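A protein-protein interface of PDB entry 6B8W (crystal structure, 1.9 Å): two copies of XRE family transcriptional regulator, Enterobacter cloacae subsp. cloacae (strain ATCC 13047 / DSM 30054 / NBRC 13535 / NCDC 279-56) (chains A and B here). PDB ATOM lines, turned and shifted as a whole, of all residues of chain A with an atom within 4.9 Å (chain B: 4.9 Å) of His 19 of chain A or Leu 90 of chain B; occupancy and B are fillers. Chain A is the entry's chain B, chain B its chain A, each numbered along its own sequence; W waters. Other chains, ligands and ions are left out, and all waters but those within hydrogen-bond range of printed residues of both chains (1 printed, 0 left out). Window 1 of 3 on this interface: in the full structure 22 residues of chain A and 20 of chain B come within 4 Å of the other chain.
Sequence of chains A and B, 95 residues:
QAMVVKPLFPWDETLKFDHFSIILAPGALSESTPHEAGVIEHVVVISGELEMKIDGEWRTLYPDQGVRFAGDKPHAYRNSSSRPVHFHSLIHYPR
Printed residues of chain B within 4 Å of His 19 of chain A: Val 44 and Leu 90. Ser 89 of chain A touches none of the printed residues of chain B. Of the printed residues of chain A, Phe 17 of chain B touches Leu 90 (3.7 Å). Of the printed residues of chain A, His 19 of chain B touches Leu 90 (3.7 Å). Printed residues of chain A within 4 Å of Leu 90 of chain B: Phe 17 (3.9 Å), His 19 (3.9 Å) and Leu 90 (3.9999 Å). Ile 91 of chain B touches none of the printed residues of chain A.
Water W1 lies within hydrogen-bond range of ND1 of His 88 of chain A (2.8 Å), ND1 of His 88 of chain B (2.9 Å) and NE2 of His 19 of chain A (3.0 Å).
The backbone carbonyl oxygen (O) of Val 44 of chain B sits at hydrogen-bond distance from the backbone NH (N) of His 88 of chain B, 2.8 Å away. N of Leu 8 of chain A lies within hydrogen-bond range of O of His 19 of chain A (2.8 Å). NE2 of His 19 of chain B sits at hydrogen-bond distance from ND1 of His 88 of chain B. O of His 42 of chain B lies within hydrogen-bond range of N of Leu 90 of chain B, 2.8 Å away.
Among the printed residues, pairs that only touch across the chains: Phe 9 of chain A with His 42 of chain B, Phe 9 of chain A with Val 44 of chain B, Phe 17 of chain A with His 42 of chain B, Phe 17 of chain A with Leu 90 of chain B, His 19 of chain A with Val 44 of chain B, His 19 of chain A with Leu 90 of chain B, His 88 of chain A with Val 44 of chain B, Leu 90 of chain A with Phe 17 of chain B, Leu 90 of chain A with His 19 of chain B and Leu 90 of chain A with Leu 90 of chain B.
Phe 17 of chain A touches Leu 90 of chain B, and with the chains exchanged Leu 90 of chain A touches Phe 17 of chain B. His 19 of chain A touches Leu 90 of chain B, and with the chains exchanged Leu 90 of chain A touches His 19 of chain B. Leu 90 of chain B touches its own counterpart, Leu 90 of chain A. Positions printed for both chains: 17, 18, 19, 88, 89 and 90.
Printed residues of chain A that touch a printed residue of chain B: Phe 9, Phe 17, His 19, His 88 and Leu 90. Of the 12 printed residues of chain B, 5 touch a printed residue of chain A. Hydrophobic or aromatic side chains of chain B within 4 Å of the printed part of chain A: Phe 17, His 19, His 42, Val 44 and Leu 90. Among the printed residues, 10 pairs touch across the chains. Among the printed residues, no Asp or Glu carboxylate lies within 4 Å of a Lys or Arg side-chain nitrogen of the other chain.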
ATOM      1  N   LYS A   6       1.085  19.767   8.436  1.00  0.00           N
ATOM      2  CA  LYS A   6      -0.221  19.117   8.415  1.00  0.00           C
ATOM      3  C   LYS A   6      -1.339  20.114   8.756  1.00  0.00           C
ATOM      4  O   LYS A   6      -1.322  20.679   9.854  1.00  0.00           O
ATOM      5  CB  LYS A   6      -0.212  17.997   9.461  1.00  0.00           C
ATOM      6  CG  LYS A   6      -1.540  17.297   9.677  1.00  0.00           C
ATOM      7  CD  LYS A   6      -1.503  16.408  10.911  1.00  0.00           C
ATOM      8  CE  LYS A   6      -2.909  15.974  11.313  1.00  0.00           C
ATOM      9  NZ  LYS A   6      -2.892  15.044  12.481  1.00  0.00           N
ATOM     10  N   PRO A   7      -2.311  20.329   7.834  1.00  0.00           N
ATOM     11  CA  PRO A   7      -3.439  21.219   8.162  1.00  0.00           C
ATOM     12  C   PRO A   7      -4.327  20.612   9.250  1.00  0.00           C
ATOM     13  O   PRO A   7      -4.735  19.469   9.131  1.00  0.00           O
ATOM     14  CB  PRO A   7      -4.228  21.306   6.848  1.00  0.00           C
ATOM     15  CG  PRO A   7      -3.869  20.076   6.103  1.00  0.00           C
ATOM     16  CD  PRO A   7      -2.446  19.760   6.479  1.00  0.00           C
ATOM     17  N   LEU A   8      -4.591  21.370  10.308  1.00  0.00           N
ATOM     18  CA  LEU A   8      -5.450  20.899  11.413  1.00  0.00           C
ATOM     19  C   LEU A   8      -6.916  20.978  11.001  1.00  0.00           C
ATOM     20  O   LEU A   8      -7.761  20.193  11.456  1.00  0.00           O
ATOM     21  CB  LEU A   8      -5.173  21.709  12.683  1.00  0.00           C
ATOM     22  CG  LEU A   8      -3.781  21.459  13.271  1.00  0.00           C
ATOM     23  CD1 LEU A   8      -3.423  22.447  14.381  1.00  0.00           C
ATOM     24  CD2 LEU A   8      -3.647  20.034  13.782  1.00  0.00           C
ATOM     25  N   PHE A   9      -7.199  21.949  10.146  1.00  0.00           N
ATOM     26  CA  PHE A   9      -8.518  22.155   9.563  1.00  0.00           C
ATOM     27  C   PHE A   9      -8.291  22.590   8.129  1.00  0.00           C
ATOM     28  O   PHE A   9      -7.251  23.193   7.824  1.00  0.00           O
ATOM     29  CB  PHE A   9      -9.288  23.269  10.269  1.00  0.00           C
ATOM     30  CG  PHE A   9      -9.605  22.962  11.700  1.00  0.00           C
ATOM     31  CD1 PHE A   9     -10.706  22.188  12.020  1.00  0.00           C
ATOM     32  CD2 PHE A   9      -8.780  23.405  12.713  1.00  0.00           C
ATOM     33  CE1 PHE A   9     -10.991  21.876  13.334  1.00  0.00           C
ATOM     34  CE2 PHE A   9      -9.055  23.093  14.035  1.00  0.00           C
ATOM     35  CZ  PHE A   9     -10.166  22.336  14.344  1.00  0.00           C
ATOM     36  N   PHE A  17      -9.108  31.880   7.437  1.00  0.00           N
ATOM     37  CA  PHE A  17      -8.171  31.360   8.415  1.00  0.00           C
ATOM     38  C   PHE A  17      -7.667  29.952   8.099  1.00  0.00           C
ATOM     39  O   PHE A  17      -8.456  29.087   7.734  1.00  0.00           O
ATOM     40  CB  PHE A  17      -8.940  31.460   9.768  1.00  0.00           C
ATOM     41  CG  PHE A  17      -8.550  30.474  10.813  1.00  0.00           C
ATOM     42  CD1 PHE A  17      -7.342  30.572  11.467  1.00  0.00           C
ATOM     43  CD2 PHE A  17      -9.473  29.511  11.240  1.00  0.00           C
ATOM     44  CE1 PHE A  17      -7.008  29.676  12.472  1.00  0.00           C
ATOM     45  CE2 PHE A  17      -9.149  28.612  12.240  1.00  0.00           C
ATOM     46  CZ  PHE A  17      -7.916  28.692  12.856  1.00  0.00           C
ATOM     47  N   ASP A  18      -6.339  29.770   8.174  1.00  0.00           N
ATOM     48  CA  ASP A  18      -5.664  28.455   8.056  1.00  0.00           C
ATOM     49  C   ASP A  18      -5.047  28.103   9.420  1.00  0.00           C
ATOM     50  O   ASP A  18      -4.627  28.980  10.171  1.00  0.00           O
ATOM     51  CB  ASP A  18      -4.519  28.458   7.034  1.00  0.00           C
ATOM     52  CG  ASP A  18      -4.966  28.186   5.619  1.00  0.00           C
ATOM     53  OD1 ASP A  18      -5.877  27.375   5.393  1.00  0.00           O
ATOM     54  OD2 ASP A  18      -4.342  28.748   4.713  1.00  0.00           O
ATOM     55  N   HIS A  19      -4.935  26.811   9.696  1.00  0.00           N
ATOM     56  CA  HIS A  19      -4.428  26.336  10.987  1.00  0.00           C
ATOM     57  C   HIS A  19      -3.598  25.106  10.703  1.00  0.00           C
ATOM     58  O   HIS A  19      -4.137  24.113  10.217  1.00  0.00           O
ATOM     59  CB  HIS A  19      -5.614  25.967  11.877  1.00  0.00           C
ATOM     60  CG  HIS A  19      -5.275  25.816  13.330  1.00  0.00           C
ATOM     61  ND1 HIS A  19      -6.238  25.570  14.285  1.00  0.00           N
ATOM     62  CD2 HIS A  19      -4.115  25.978  14.004  1.00  0.00           C
ATOM     63  CE1 HIS A  19      -5.676  25.534  15.479  1.00  0.00           C
ATOM     64  NE2 HIS A  19      -4.385  25.768  15.336  1.00  0.00           N
ATOM     65  N   PHE A  20      -2.300  25.161  11.002  1.00  0.00           N
ATOM     66  CA  PHE A  20      -1.370  24.069  10.691  1.00  0.00           C
ATOM     67  C   PHE A  20      -0.595  23.551  11.888  1.00  0.00           C
ATOM     68  O   PHE A  20      -0.339  24.281  12.831  1.00  0.00           O
ATOM     69  CB  PHE A  20      -0.290  24.545   9.698  1.00  0.00           C
ATOM     70  CG  PHE A  20      -0.819  25.034   8.390  1.00  0.00           C
ATOM     71  CD1 PHE A  20      -1.168  24.134   7.389  1.00  0.00           C
ATOM     72  CD2 PHE A  20      -0.913  26.397   8.126  1.00  0.00           C
ATOM     73  CE1 PHE A  20      -1.645  24.580   6.166  1.00  0.00           C
ATOM     74  CE2 PHE A  20      -1.374  26.851   6.897  1.00  0.00           C
ATOM     75  CZ  PHE A  20      -1.749  25.942   5.920  1.00  0.00           C
ATOM     76  N   SER A  21      -0.198  22.284  11.801  1.00  0.00           N
ATOM     77  CA  SER A  21       0.705  21.662  12.753  1.00  0.00           C
ATOM     78  C   SER A  21       1.985  21.429  11.980  1.00  0.00           C
ATOM     79  O   SER A  21       1.939  20.956  10.830  1.00  0.00           O
ATOM     80  CB  SER A  21       0.185  20.325  13.236  1.00  0.00           C
ATOM     81  OG  SER A  21       1.129  19.733  14.092  1.00  0.00           O
ATOM     82  N   HIS A  88       2.154  24.774  16.431  1.00  0.00           N
ATOM     83  CA  HIS A  88       1.010  25.131  15.606  1.00  0.00           C
ATOM     84  C   HIS A  88       1.207  26.519  15.068  1.00  0.00           C
ATOM     85  O   HIS A  88       1.769  27.375  15.750  1.00  0.00           O
ATOM     86  CB  HIS A  88      -0.310  25.054  16.359  1.00  0.00           C
ATOM     87  CG  HIS A  88      -0.707  23.663  16.735  1.00  0.00           C
ATOM     88  ND1 HIS A  88      -1.812  23.390  17.507  1.00  0.00           N
ATOM     89  CD2 HIS A  88      -0.125  22.466  16.477  1.00  0.00           C
ATOM     90  CE1 HIS A  88      -1.924  22.087  17.665  1.00  0.00           C
ATOM     91  NE2 HIS A  88      -0.922  21.500  17.043  1.00  0.00           N
ATOM     92  N   SER A  89       0.731  26.731  13.846  1.00  0.00           N
ATOM     93  CA  SER A  89       0.800  28.018  13.188  1.00  0.00           C
ATOM     94  C   SER A  89      -0.605  28.401  12.711  1.00  0.00           C
ATOM     95  O   SER A  89      -1.258  27.615  12.022  1.00  0.00           O
ATOM     96  CB  SER A  89       1.756  27.930  12.003  1.00  0.00           C
ATOM     97  OG  SER A  89       1.820  29.159  11.296  1.00  0.00           O
ATOM     98  N   LEU A  90      -1.081  29.576  13.115  1.00  0.00           N
ATOM     99  CA  LEU A  90      -2.381  30.081  12.678  1.00  0.00           C
ATOM    100  C   LEU A  90      -2.126  31.207  11.706  1.00  0.00           C
ATOM    101  O   LEU A  90      -1.215  31.980  11.919  1.00  0.00           O
ATOM    102  CB  LEU A  90      -3.197  30.620  13.853  1.00  0.00           C
ATOM    103  CG  LEU A  90      -3.744  29.657  14.889  1.00  0.00           C
ATOM    104  CD1 LEU A  90      -2.644  28.852  15.562  1.00  0.00           C
ATOM    105  CD2 LEU A  90      -4.530  30.435  15.928  1.00  0.00           C
ATOM    106  N   PHE B  17     -11.119  37.577  18.187  1.00  0.00           N
ATOM    107  CA  PHE B  17     -10.644  36.210  18.368  1.00  0.00           C
ATOM    108  C   PHE B  17     -10.008  35.968  19.736  1.00  0.00           C
ATOM    109  O   PHE B  17      -9.227  36.781  20.215  1.00  0.00           O
ATOM    110  CB  PHE B  17      -9.635  35.958  17.224  1.00  0.00           C
ATOM    111  CG  PHE B  17      -8.781  34.726  17.379  1.00  0.00           C
ATOM    112  CD1 PHE B  17      -9.328  33.462  17.248  1.00  0.00           C
ATOM    113  CD2 PHE B  17      -7.394  34.837  17.564  1.00  0.00           C
ATOM    114  CE1 PHE B  17      -8.531  32.321  17.361  1.00  0.00           C
ATOM    115  CE2 PHE B  17      -6.595  33.701  17.663  1.00  0.00           C
ATOM    116  CZ  PHE B  17      -7.162  32.443  17.559  1.00  0.00           C
ATOM    117  N   ASP B  18     -10.419  34.871  20.372  1.00  0.00           N
ATOM    118  CA  ASP B  18      -9.851  34.403  21.626  1.00  0.00           C
ATOM    119  C   ASP B  18      -9.240  33.039  21.363  1.00  0.00           C
ATOM    120  O   ASP B  18      -9.684  32.296  20.497  1.00  0.00           O
ATOM    121  CB  ASP B  18     -10.910  34.306  22.740  1.00  0.00           C
ATOM    122  CG  ASP B  18     -10.941  35.517  23.651  1.00  0.00           C
ATOM    123  OD1 ASP B  18      -9.882  36.148  23.876  1.00  0.00           O
ATOM    124  OD2 ASP B  18     -12.032  35.799  24.206  1.00  0.00           O
ATOM    125  N   HIS B  19      -8.227  32.709  22.137  1.00  0.00           N
ATOM    126  CA  HIS B  19      -7.493  31.463  21.980  1.00  0.00           C
ATOM    127  C   HIS B  19      -7.138  31.029  23.413  1.00  0.00           C
ATOM    128  O   HIS B  19      -6.311  31.663  24.080  1.00  0.00           O
ATOM    129  CB  HIS B  19      -6.234  31.754  21.179  1.00  0.00           C
ATOM    130  CG  HIS B  19      -5.510  30.543  20.708  1.00  0.00           C
ATOM    131  ND1 HIS B  19      -4.683  30.563  19.611  1.00  0.00           N
ATOM    132  CD2 HIS B  19      -5.539  29.260  21.133  1.00  0.00           C
ATOM    133  CE1 HIS B  19      -4.199  29.348  19.405  1.00  0.00           C
ATOM    134  NE2 HIS B  19      -4.693  28.542  20.322  1.00  0.00           N
ATOM    135  N   ILE B  40     -18.178  31.030  16.342  1.00  0.00           N
ATOM    136  CA  ILE B  40     -17.624  29.770  15.880  1.00  0.00           C
ATOM    137  C   ILE B  40     -16.531  29.365  16.873  1.00  0.00           C
ATOM    138  O   ILE B  40     -15.740  30.195  17.288  1.00  0.00           O
ATOM    139  CB  ILE B  40     -17.025  29.849  14.476  1.00  0.00           C
ATOM    140  CG1 ILE B  40     -18.062  30.297  13.454  1.00  0.00           C
ATOM    141  CG2 ILE B  40     -16.421  28.490  14.072  1.00  0.00           C
ATOM    142  CD1 ILE B  40     -19.240  29.347  13.265  1.00  0.00           C
ATOM    143  N   GLU B  41     -16.530  28.091  17.253  1.00  0.00           N
ATOM    144  CA  GLU B  41     -15.528  27.531  18.122  1.00  0.00           C
ATOM    145  C   GLU B  41     -14.763  26.383  17.423  1.00  0.00           C
ATOM    146  O   GLU B  41     -15.344  25.599  16.654  1.00  0.00           O
ATOM    147  CB  GLU B  41     -16.130  27.054  19.453  1.00  0.00           C
ATOM    148  CG  GLU B  41     -15.100  26.392  20.369  1.00  0.00           C
ATOM    149  CD  GLU B  41     -15.536  26.140  21.812  1.00  0.00           C
ATOM    150  OE1 GLU B  41     -16.664  26.523  22.214  1.00  0.00           O
ATOM    151  OE2 GLU B  41     -14.714  25.533  22.557  1.00  0.00           O
ATOM    152  N   HIS B  42     -13.449  26.340  17.656  1.00  0.00           N
ATOM    153  CA  HIS B  42     -12.606  25.235  17.192  1.00  0.00           C
ATOM    154  C   HIS B  42     -11.993  24.636  18.457  1.00  0.00           C
ATOM    155  O   HIS B  42     -11.536  25.357  19.330  1.00  0.00           O
ATOM    156  CB  HIS B  42     -11.424  25.682  16.306  1.00  0.00           C
ATOM    157  CG  HIS B  42     -11.790  26.178  14.944  1.00  0.00           C
ATOM    158  ND1 HIS B  42     -12.278  27.446  14.718  1.00  0.00           N
ATOM    159  CD2 HIS B  42     -11.669  25.599  13.721  1.00  0.00           C
ATOM    160  CE1 HIS B  42     -12.469  27.620  13.422  1.00  0.00           C
ATOM    161  NE2 HIS B  42     -12.107  26.514  12.792  1.00  0.00           N
ATOM    162  N   VAL B  44      -9.034  21.820  19.423  1.00  0.00           N
ATOM    163  CA  VAL B  44      -7.921  21.008  18.938  1.00  0.00           C
ATOM    164  C   VAL B  44      -7.273  20.383  20.161  1.00  0.00           C
ATOM    165  O   VAL B  44      -6.942  21.088  21.120  1.00  0.00           O
ATOM    166  CB  VAL B  44      -6.859  21.844  18.192  1.00  0.00           C
ATOM    167  CG1 VAL B  44      -5.672  20.971  17.786  1.00  0.00           C
ATOM    168  CG2 VAL B  44      -7.468  22.520  16.975  1.00  0.00           C
ATOM    169  N   HIS B  88      -6.903  23.156  23.047  1.00  0.00           N
ATOM    170  CA  HIS B  88      -7.099  24.575  22.801  1.00  0.00           C
ATOM    171  C   HIS B  88      -8.508  24.789  22.331  1.00  0.00           C
ATOM    172  O   HIS B  88      -9.072  23.952  21.610  1.00  0.00           O
ATOM    173  CB  HIS B  88      -6.193  25.172  21.720  1.00  0.00           C
ATOM    174  CG  HIS B  88      -4.740  25.170  22.042  1.00  0.00           C
ATOM    175  ND1 HIS B  88      -3.782  25.476  21.095  1.00  0.00           N
ATOM    176  CD2 HIS B  88      -4.068  24.863  23.174  1.00  0.00           C
ATOM    177  CE1 HIS B  88      -2.586  25.383  21.642  1.00  0.00           C
ATOM    178  NE2 HIS B  88      -2.727  24.998  22.896  1.00  0.00           N
ATOM    179  N   SER B  89      -9.066  25.924  22.731  1.00  0.00           N
ATOM    180  CA  SER B  89     -10.387  26.338  22.320  1.00  0.00           C
ATOM    181  C   SER B  89     -10.218  27.693  21.664  1.00  0.00           C
ATOM    182  O   SER B  89      -9.785  28.642  22.304  1.00  0.00           O
ATOM    183  CB  SER B  89     -11.324  26.416  23.522  1.00  0.00           C
ATOM    184  OG  SER B  89     -12.531  27.078  23.180  1.00  0.00           O
ATOM    185  N   LEU B  90     -10.525  27.766  20.374  1.00  0.00           N
ATOM    186  CA  LEU B  90     -10.437  29.006  19.627  1.00  0.00           C
ATOM    187  C   LEU B  90     -11.841  29.514  19.408  1.00  0.00           C
ATOM    188  O   LEU B  90     -12.722  28.747  19.041  1.00  0.00           O
ATOM    189  CB  LEU B  90      -9.779  28.784  18.272  1.00  0.00           C
ATOM    190  CG  LEU B  90      -8.283  28.444  18.241  1.00  0.00           C
ATOM    191  CD1 LEU B  90      -7.971  27.115  18.884  1.00  0.00           C
ATOM    192  CD2 LEU B  90      -7.875  28.414  16.780  1.00  0.00           C
ATOM    193  N   ILE B  91     -12.040  30.805  19.624  1.00  0.00           N
ATOM    194  CA  ILE B  91     -13.352  31.411  19.468  1.00  0.00           C
ATOM    195  C   ILE B  91     -13.284  32.593  18.521  1.00  0.00           C
ATOM    196  O   ILE B  91     -12.510  33.492  18.752  1.00  0.00           O
ATOM    197  CB  ILE B  91     -13.894  31.924  20.818  1.00  0.00           C
ATOM    198  CG1 ILE B  91     -13.967  30.799  21.872  1.00  0.00           C
ATOM    199  CG2 ILE B  91     -15.250  32.586  20.617  1.00  0.00           C
ATOM    200  CD1 ILE B  91     -15.028  29.742  21.616  1.00  0.00           C
ATOM    201  N   HIS B  92     -14.075  32.559  17.450  1.00  0.00           N
ATOM    202  CA  HIS B  92     -14.200  33.684  16.522  1.00  0.00           C
ATOM    203  C   HIS B  92     -15.597  34.294  16.752  1.00  0.00           C
ATOM    204  O   HIS B  92     -16.620  33.617  16.572  1.00  0.00           O
ATOM    205  CB  HIS B  92     -14.015  33.239  15.067  1.00  0.00           C
ATOM    206  CG  HIS B  92     -12.592  32.970  14.695  1.00  0.00           C
ATOM    207  ND1 HIS B  92     -11.961  31.779  14.976  1.00  0.00           N
ATOM    208  CD2 HIS B  92     -11.675  33.744  14.061  1.00  0.00           C
ATOM    209  CE1 HIS B  92     -10.710  31.839  14.546  1.00  0.00           C
ATOM    210  NE2 HIS B  92     -10.514  33.018  13.982  1.00  0.00           N
HETATM  211  O   HOH W   1      -3.518  25.516  18.191  1.00  0.00           O
